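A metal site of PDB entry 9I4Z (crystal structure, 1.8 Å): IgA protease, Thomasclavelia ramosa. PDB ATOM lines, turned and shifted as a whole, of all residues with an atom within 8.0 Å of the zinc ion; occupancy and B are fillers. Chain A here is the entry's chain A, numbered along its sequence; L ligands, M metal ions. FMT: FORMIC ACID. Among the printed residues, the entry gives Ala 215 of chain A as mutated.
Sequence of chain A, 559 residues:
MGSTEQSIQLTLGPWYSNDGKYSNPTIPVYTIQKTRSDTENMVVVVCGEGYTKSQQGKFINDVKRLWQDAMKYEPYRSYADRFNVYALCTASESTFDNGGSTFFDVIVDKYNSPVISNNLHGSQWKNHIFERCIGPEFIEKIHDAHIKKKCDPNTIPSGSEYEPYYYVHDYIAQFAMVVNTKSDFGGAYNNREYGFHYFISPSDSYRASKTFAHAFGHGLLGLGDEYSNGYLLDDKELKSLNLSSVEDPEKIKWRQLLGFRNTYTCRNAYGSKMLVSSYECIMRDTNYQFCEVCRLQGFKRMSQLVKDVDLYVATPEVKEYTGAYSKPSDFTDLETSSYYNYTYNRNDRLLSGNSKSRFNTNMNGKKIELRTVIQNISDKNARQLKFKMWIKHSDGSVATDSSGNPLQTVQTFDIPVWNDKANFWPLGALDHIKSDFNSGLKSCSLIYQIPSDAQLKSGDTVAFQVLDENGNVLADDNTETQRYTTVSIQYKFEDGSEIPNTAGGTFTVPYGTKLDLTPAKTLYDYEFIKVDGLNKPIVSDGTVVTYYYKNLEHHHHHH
Of the 19 residues printed, 3 come within 4 Å of the zinc ion.
The zinc ion is bound by NE2 of His 218, OD2 of Asp 225, NE2 of His 214, O2 of the ligand and O1 of the ligand.
The zinc ion has five donor atoms within binding distance.
ND1 of His 218 is in hydrogen-bond range of O of Leu 223 (2.7 Å).
O of Asp 225 sits at hydrogen-bond distance from OG of Ser 228 (2.7 Å).
The backbone carbonyl oxygen of Ile 282 is in hydrogen-bond range of a ring nitrogen (ND1) of His 214 (2.8 Å).
OD1 of Asp 225 is in hydrogen-bond range of OH of Tyr 227 (3.2 Å).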
ATOM      1  N   GLY A 186       9.670 -33.990  -5.351  1.00  0.00           N
ATOM      2  CA  GLY A 186      10.484 -33.620  -6.505  1.00  0.00           C
ATOM      3  C   GLY A 186      10.944 -32.195  -6.349  1.00  0.00           C
ATOM      4  O   GLY A 186      10.206 -31.364  -5.805  1.00  0.00           O
ATOM      5  N   GLY A 187      12.195 -31.919  -6.726  1.00  0.00           N
ATOM      6  CA  GLY A 187      12.724 -30.574  -6.591  1.00  0.00           C
ATOM      7  C   GLY A 187      13.789 -30.273  -7.628  1.00  0.00           C
ATOM      8  O   GLY A 187      14.681 -31.075  -7.821  1.00  0.00           O
ATOM      9  N   ALA A 188      13.686 -29.128  -8.303  1.00  0.00           N
ATOM     10  CA  ALA A 188      14.614 -28.737  -9.345  1.00  0.00           C
ATOM     11  C   ALA A 188      15.355 -27.498  -8.904  1.00  0.00           C
ATOM     12  O   ALA A 188      14.728 -26.553  -8.422  1.00  0.00           O
ATOM     13  CB  ALA A 188      13.840 -28.468 -10.625  1.00  0.00           C
ATOM     14  N   THR A 211       7.962 -37.971 -12.362  1.00  0.00           N
ATOM     15  CA  THR A 211       8.643 -36.885 -11.646  1.00  0.00           C
ATOM     16  C   THR A 211      10.031 -36.596 -12.264  1.00  0.00           C
ATOM     17  O   THR A 211      10.410 -35.451 -12.474  1.00  0.00           O
ATOM     18  CB  THR A 211       8.795 -37.262 -10.158  1.00  0.00           C
ATOM     19  OG1 THR A 211       7.513 -37.350  -9.572  1.00  0.00           O
ATOM     20  CG2 THR A 211       9.614 -36.233  -9.406  1.00  0.00           C
ATOM     21  N   HIS A 214       9.654 -34.750 -15.573  1.00  0.00           N
ATOM     22  CA  HIS A 214       9.240 -33.362 -15.292  1.00  0.00           C
ATOM     23  C   HIS A 214      10.440 -32.516 -14.801  1.00  0.00           C
ATOM     24  O   HIS A 214      10.697 -31.410 -15.310  1.00  0.00           O
ATOM     25  CB  HIS A 214       8.105 -33.379 -14.241  1.00  0.00           C
ATOM     26  CG  HIS A 214       7.717 -32.024 -13.719  1.00  0.00           C
ATOM     27  ND1 HIS A 214       6.643 -31.332 -14.233  1.00  0.00           N
ATOM     28  CD2 HIS A 214       8.283 -31.291 -12.739  1.00  0.00           C
ATOM     29  CE1 HIS A 214       6.582 -30.195 -13.564  1.00  0.00           C
ATOM     30  NE2 HIS A 214       7.548 -30.116 -12.652  1.00  0.00           N
ATOM     31  N   ALA A 215      11.176 -33.009 -13.781  1.00  0.00           N
ATOM     32  CA  ALA A 215      12.325 -32.274 -13.241  1.00  0.00           C
ATOM     33  C   ALA A 215      13.423 -32.088 -14.303  1.00  0.00           C
ATOM     34  O   ALA A 215      14.068 -31.035 -14.365  1.00  0.00           O
ATOM     35  CB  ALA A 215      12.895 -33.025 -12.033  1.00  0.00           C
ATOM     36  N   PHE A 216      13.632 -33.087 -15.142  1.00  0.00           N
ATOM     37  CA  PHE A 216      14.583 -33.009 -16.250  1.00  0.00           C
ATOM     38  C   PHE A 216      14.093 -31.911 -17.286  1.00  0.00           C
ATOM     39  O   PHE A 216      14.908 -31.265 -17.939  1.00  0.00           O
ATOM     40  CB  PHE A 216      14.701 -34.414 -16.870  1.00  0.00           C
ATOM     41  CG  PHE A 216      15.917 -34.738 -17.707  1.00  0.00           C
ATOM     42  CD1 PHE A 216      17.119 -34.098 -17.490  1.00  0.00           C
ATOM     43  CD2 PHE A 216      15.859 -35.752 -18.654  1.00  0.00           C
ATOM     44  CE1 PHE A 216      18.238 -34.426 -18.253  1.00  0.00           C
ATOM     45  CE2 PHE A 216      16.989 -36.059 -19.423  1.00  0.00           C
ATOM     46  CZ  PHE A 216      18.170 -35.401 -19.217  1.00  0.00           C
ATOM     47  N   GLY A 217      12.776 -31.690 -17.376  1.00  0.00           N
ATOM     48  CA  GLY A 217      12.178 -30.654 -18.203  1.00  0.00           C
ATOM     49  C   GLY A 217      12.615 -29.267 -17.754  1.00  0.00           C
ATOM     50  O   GLY A 217      12.861 -28.384 -18.581  1.00  0.00           O
ATOM     51  N   HIS A 218      12.808 -29.077 -16.421  1.00  0.00           N
ATOM     52  CA  HIS A 218      13.331 -27.783 -15.925  1.00  0.00           C
ATOM     53  C   HIS A 218      14.848 -27.667 -16.209  1.00  0.00           C
ATOM     54  O   HIS A 218      15.312 -26.651 -16.684  1.00  0.00           O
ATOM     55  CB  HIS A 218      13.124 -27.631 -14.398  1.00  0.00           C
ATOM     56  CG  HIS A 218      11.712 -27.586 -13.933  1.00  0.00           C
ATOM     57  ND1 HIS A 218      10.826 -26.651 -14.419  1.00  0.00           N
ATOM     58  CD2 HIS A 218      11.104 -28.309 -12.963  1.00  0.00           C
ATOM     59  CE1 HIS A 218       9.694 -26.859 -13.767  1.00  0.00           C
ATOM     60  NE2 HIS A 218       9.837 -27.819 -12.846  1.00  0.00           N
ATOM     61  N   LEU A 223      12.383 -25.467 -19.189  1.00  0.00           N
ATOM     62  CA  LEU A 223      10.946 -25.172 -19.132  1.00  0.00           C
ATOM     63  C   LEU A 223      10.487 -24.748 -17.729  1.00  0.00           C
ATOM     64  O   LEU A 223      11.059 -25.175 -16.726  1.00  0.00           O
ATOM     65  CB  LEU A 223      10.149 -26.384 -19.595  1.00  0.00           C
ATOM     66  CG  LEU A 223      10.562 -26.949 -20.959  1.00  0.00           C
ATOM     67  CD1 LEU A 223      10.017 -28.377 -21.161  1.00  0.00           C
ATOM     68  CD2 LEU A 223      10.147 -26.018 -22.120  1.00  0.00           C
ATOM     69  N   GLY A 224       9.432 -23.960 -17.677  1.00  0.00           N
ATOM     70  CA  GLY A 224       8.855 -23.538 -16.411  1.00  0.00           C
ATOM     71  C   GLY A 224       7.678 -24.388 -15.993  1.00  0.00           C
ATOM     72  O   GLY A 224       7.082 -25.110 -16.811  1.00  0.00           O
ATOM     73  N   ASP A 225       7.341 -24.339 -14.687  1.00  0.00           N
ATOM     74  CA  ASP A 225       6.163 -25.013 -14.146  1.00  0.00           C
ATOM     75  C   ASP A 225       4.912 -24.365 -14.765  1.00  0.00           C
ATOM     76  O   ASP A 225       4.717 -23.147 -14.653  1.00  0.00           O
ATOM     77  CB  ASP A 225       6.109 -24.901 -12.612  1.00  0.00           C
ATOM     78  CG  ASP A 225       7.035 -25.874 -11.911  1.00  0.00           C
ATOM     79  OD1 ASP A 225       7.721 -25.456 -10.976  1.00  0.00           O
ATOM     80  OD2 ASP A 225       7.058 -27.053 -12.306  1.00  0.00           O
ATOM     81  N   GLU A 226       4.078 -25.163 -15.427  1.00  0.00           N
ATOM     82  CA  GLU A 226       2.859 -24.628 -16.037  1.00  0.00           C
ATOM     83  C   GLU A 226       1.725 -24.443 -15.028  1.00  0.00           C
ATOM     84  O   GLU A 226       0.655 -23.986 -15.427  1.00  0.00           O
ATOM     85  CB  GLU A 226       2.435 -25.484 -17.228  1.00  0.00           C
ATOM     86  CG  GLU A 226       3.464 -25.335 -18.340  1.00  0.00           C
ATOM     87  CD  GLU A 226       3.101 -26.044 -19.636  1.00  0.00           C
ATOM     88  OE1 GLU A 226       1.943 -26.510 -19.751  1.00  0.00           O
ATOM     89  OE2 GLU A 226       3.983 -26.143 -20.529  1.00  0.00           O
ATOM     90  N   TYR A 227       1.948 -24.754 -13.738  1.00  0.00           N
ATOM     91  CA  TYR A 227       0.985 -24.422 -12.685  1.00  0.00           C
ATOM     92  C   TYR A 227       1.398 -23.070 -11.994  1.00  0.00           C
ATOM     93  O   TYR A 227       0.768 -22.661 -11.011  1.00  0.00           O
ATOM     94  CB  TYR A 227       0.843 -25.570 -11.667  1.00  0.00           C
ATOM     95  CG  TYR A 227       2.135 -25.934 -10.963  1.00  0.00           C
ATOM     96  CD1 TYR A 227       2.548 -25.238  -9.833  1.00  0.00           C
ATOM     97  CD2 TYR A 227       2.918 -26.994 -11.399  1.00  0.00           C
ATOM     98  CE1 TYR A 227       3.719 -25.557  -9.174  1.00  0.00           C
ATOM     99  CE2 TYR A 227       4.090 -27.351 -10.720  1.00  0.00           C
ATOM    100  CZ  TYR A 227       4.507 -26.600  -9.638  1.00  0.00           C
ATOM    101  OH  TYR A 227       5.656 -26.924  -8.943  1.00  0.00           O
ATOM    102  N   SER A 228       2.447 -22.363 -12.529  1.00  0.00           N
ATOM    103  CA  SER A 228       2.939 -21.090 -11.979  1.00  0.00           C
ATOM    104  C   SER A 228       1.843 -20.035 -11.873  1.00  0.00           C
ATOM    105  O   SER A 228       0.910 -20.008 -12.660  1.00  0.00           O
ATOM    106  CB  SER A 228       4.079 -20.553 -12.858  1.00  0.00           C
ATOM    107  OG  SER A 228       5.221 -21.370 -12.680  1.00  0.00           O
ATOM    108  N   ILE A 282       2.853 -32.248 -19.085  1.00  0.00           N
ATOM    109  CA  ILE A 282       3.613 -32.801 -17.949  1.00  0.00           C
ATOM    110  C   ILE A 282       4.212 -31.671 -17.083  1.00  0.00           C
ATOM    111  O   ILE A 282       4.436 -31.896 -15.905  1.00  0.00           O
ATOM    112  CB  ILE A 282       4.748 -33.727 -18.483  1.00  0.00           C
ATOM    113  CG1 ILE A 282       5.291 -34.640 -17.355  1.00  0.00           C
ATOM    114  CG2 ILE A 282       5.874 -32.895 -19.133  1.00  0.00           C
ATOM    115  CD1 ILE A 282       6.464 -35.572 -17.781  1.00  0.00           C
ATOM    116  N   MET A 283       4.440 -30.463 -17.669  1.00  0.00           N
ATOM    117  CA  MET A 283       4.994 -29.375 -16.882  1.00  0.00           C
ATOM    118  C   MET A 283       3.947 -28.736 -15.924  1.00  0.00           C
ATOM    119  O   MET A 283       4.317 -27.974 -15.032  1.00  0.00           O
ATOM    120  CB  MET A 283       5.695 -28.354 -17.774  1.00  0.00           C
ATOM    121  CG  MET A 283       6.914 -28.969 -18.557  1.00  0.00           C
ATOM    122  SD  MET A 283       8.103 -29.871 -17.502  1.00  0.00           S
ATOM    123  CE  MET A 283       8.668 -28.525 -16.374  1.00  0.00           C
ATOM    124  N   ARG A 284       2.655 -29.092 -16.082  1.00  0.00           N
ATOM    125  CA  ARG A 284       1.615 -28.662 -15.173  1.00  0.00           C
ATOM    126  C   ARG A 284       1.224 -29.839 -14.304  1.00  0.00           C
ATOM    127  O   ARG A 284       1.071 -29.676 -13.098  1.00  0.00           O
ATOM    128  CB  ARG A 284       0.392 -28.139 -15.958  1.00  0.00           C
ATOM    129  CG  ARG A 284      -0.669 -27.457 -15.069  1.00  0.00           C
ATOM    130  CD  ARG A 284      -2.006 -27.139 -15.768  1.00  0.00           C
ATOM    131  NE  ARG A 284      -2.634 -28.324 -16.356  1.00  0.00           N
ATOM    132  CZ  ARG A 284      -3.344 -29.218 -15.678  1.00  0.00           C
ATOM    133  NH1 ARG A 284      -3.517 -29.092 -14.372  1.00  0.00           N
ATOM    134  NH2 ARG A 284      -3.854 -30.276 -16.304  1.00  0.00           N
ATOM    135  N   THR A 286       1.998 -34.166 -13.861  1.00  0.00           N
ATOM    136  CA  THR A 286       2.931 -35.228 -14.277  1.00  0.00           C
ATOM    137  C   THR A 286       2.291 -36.416 -14.993  1.00  0.00           C
ATOM    138  O   THR A 286       3.004 -37.285 -15.459  1.00  0.00           O
ATOM    139  CB  THR A 286       3.757 -35.730 -13.065  1.00  0.00           C
ATOM    140  OG1 THR A 286       2.857 -36.075 -12.013  1.00  0.00           O
ATOM    141  CG2 THR A 286       4.748 -34.685 -12.581  1.00  0.00           C
HETATM  142  C   FMT L   1       8.752 -29.303  -9.441  1.00  0.00           C
HETATM  143  O1  FMT L   1       9.558 -29.668 -10.319  1.00  0.00           O
HETATM  144  O2  FMT L   1       7.547 -28.646  -9.680  1.00  0.00           O
HETATM  145 ZN    ZN M   1       8.340 -28.504 -11.636  1.00  0.00          ZN
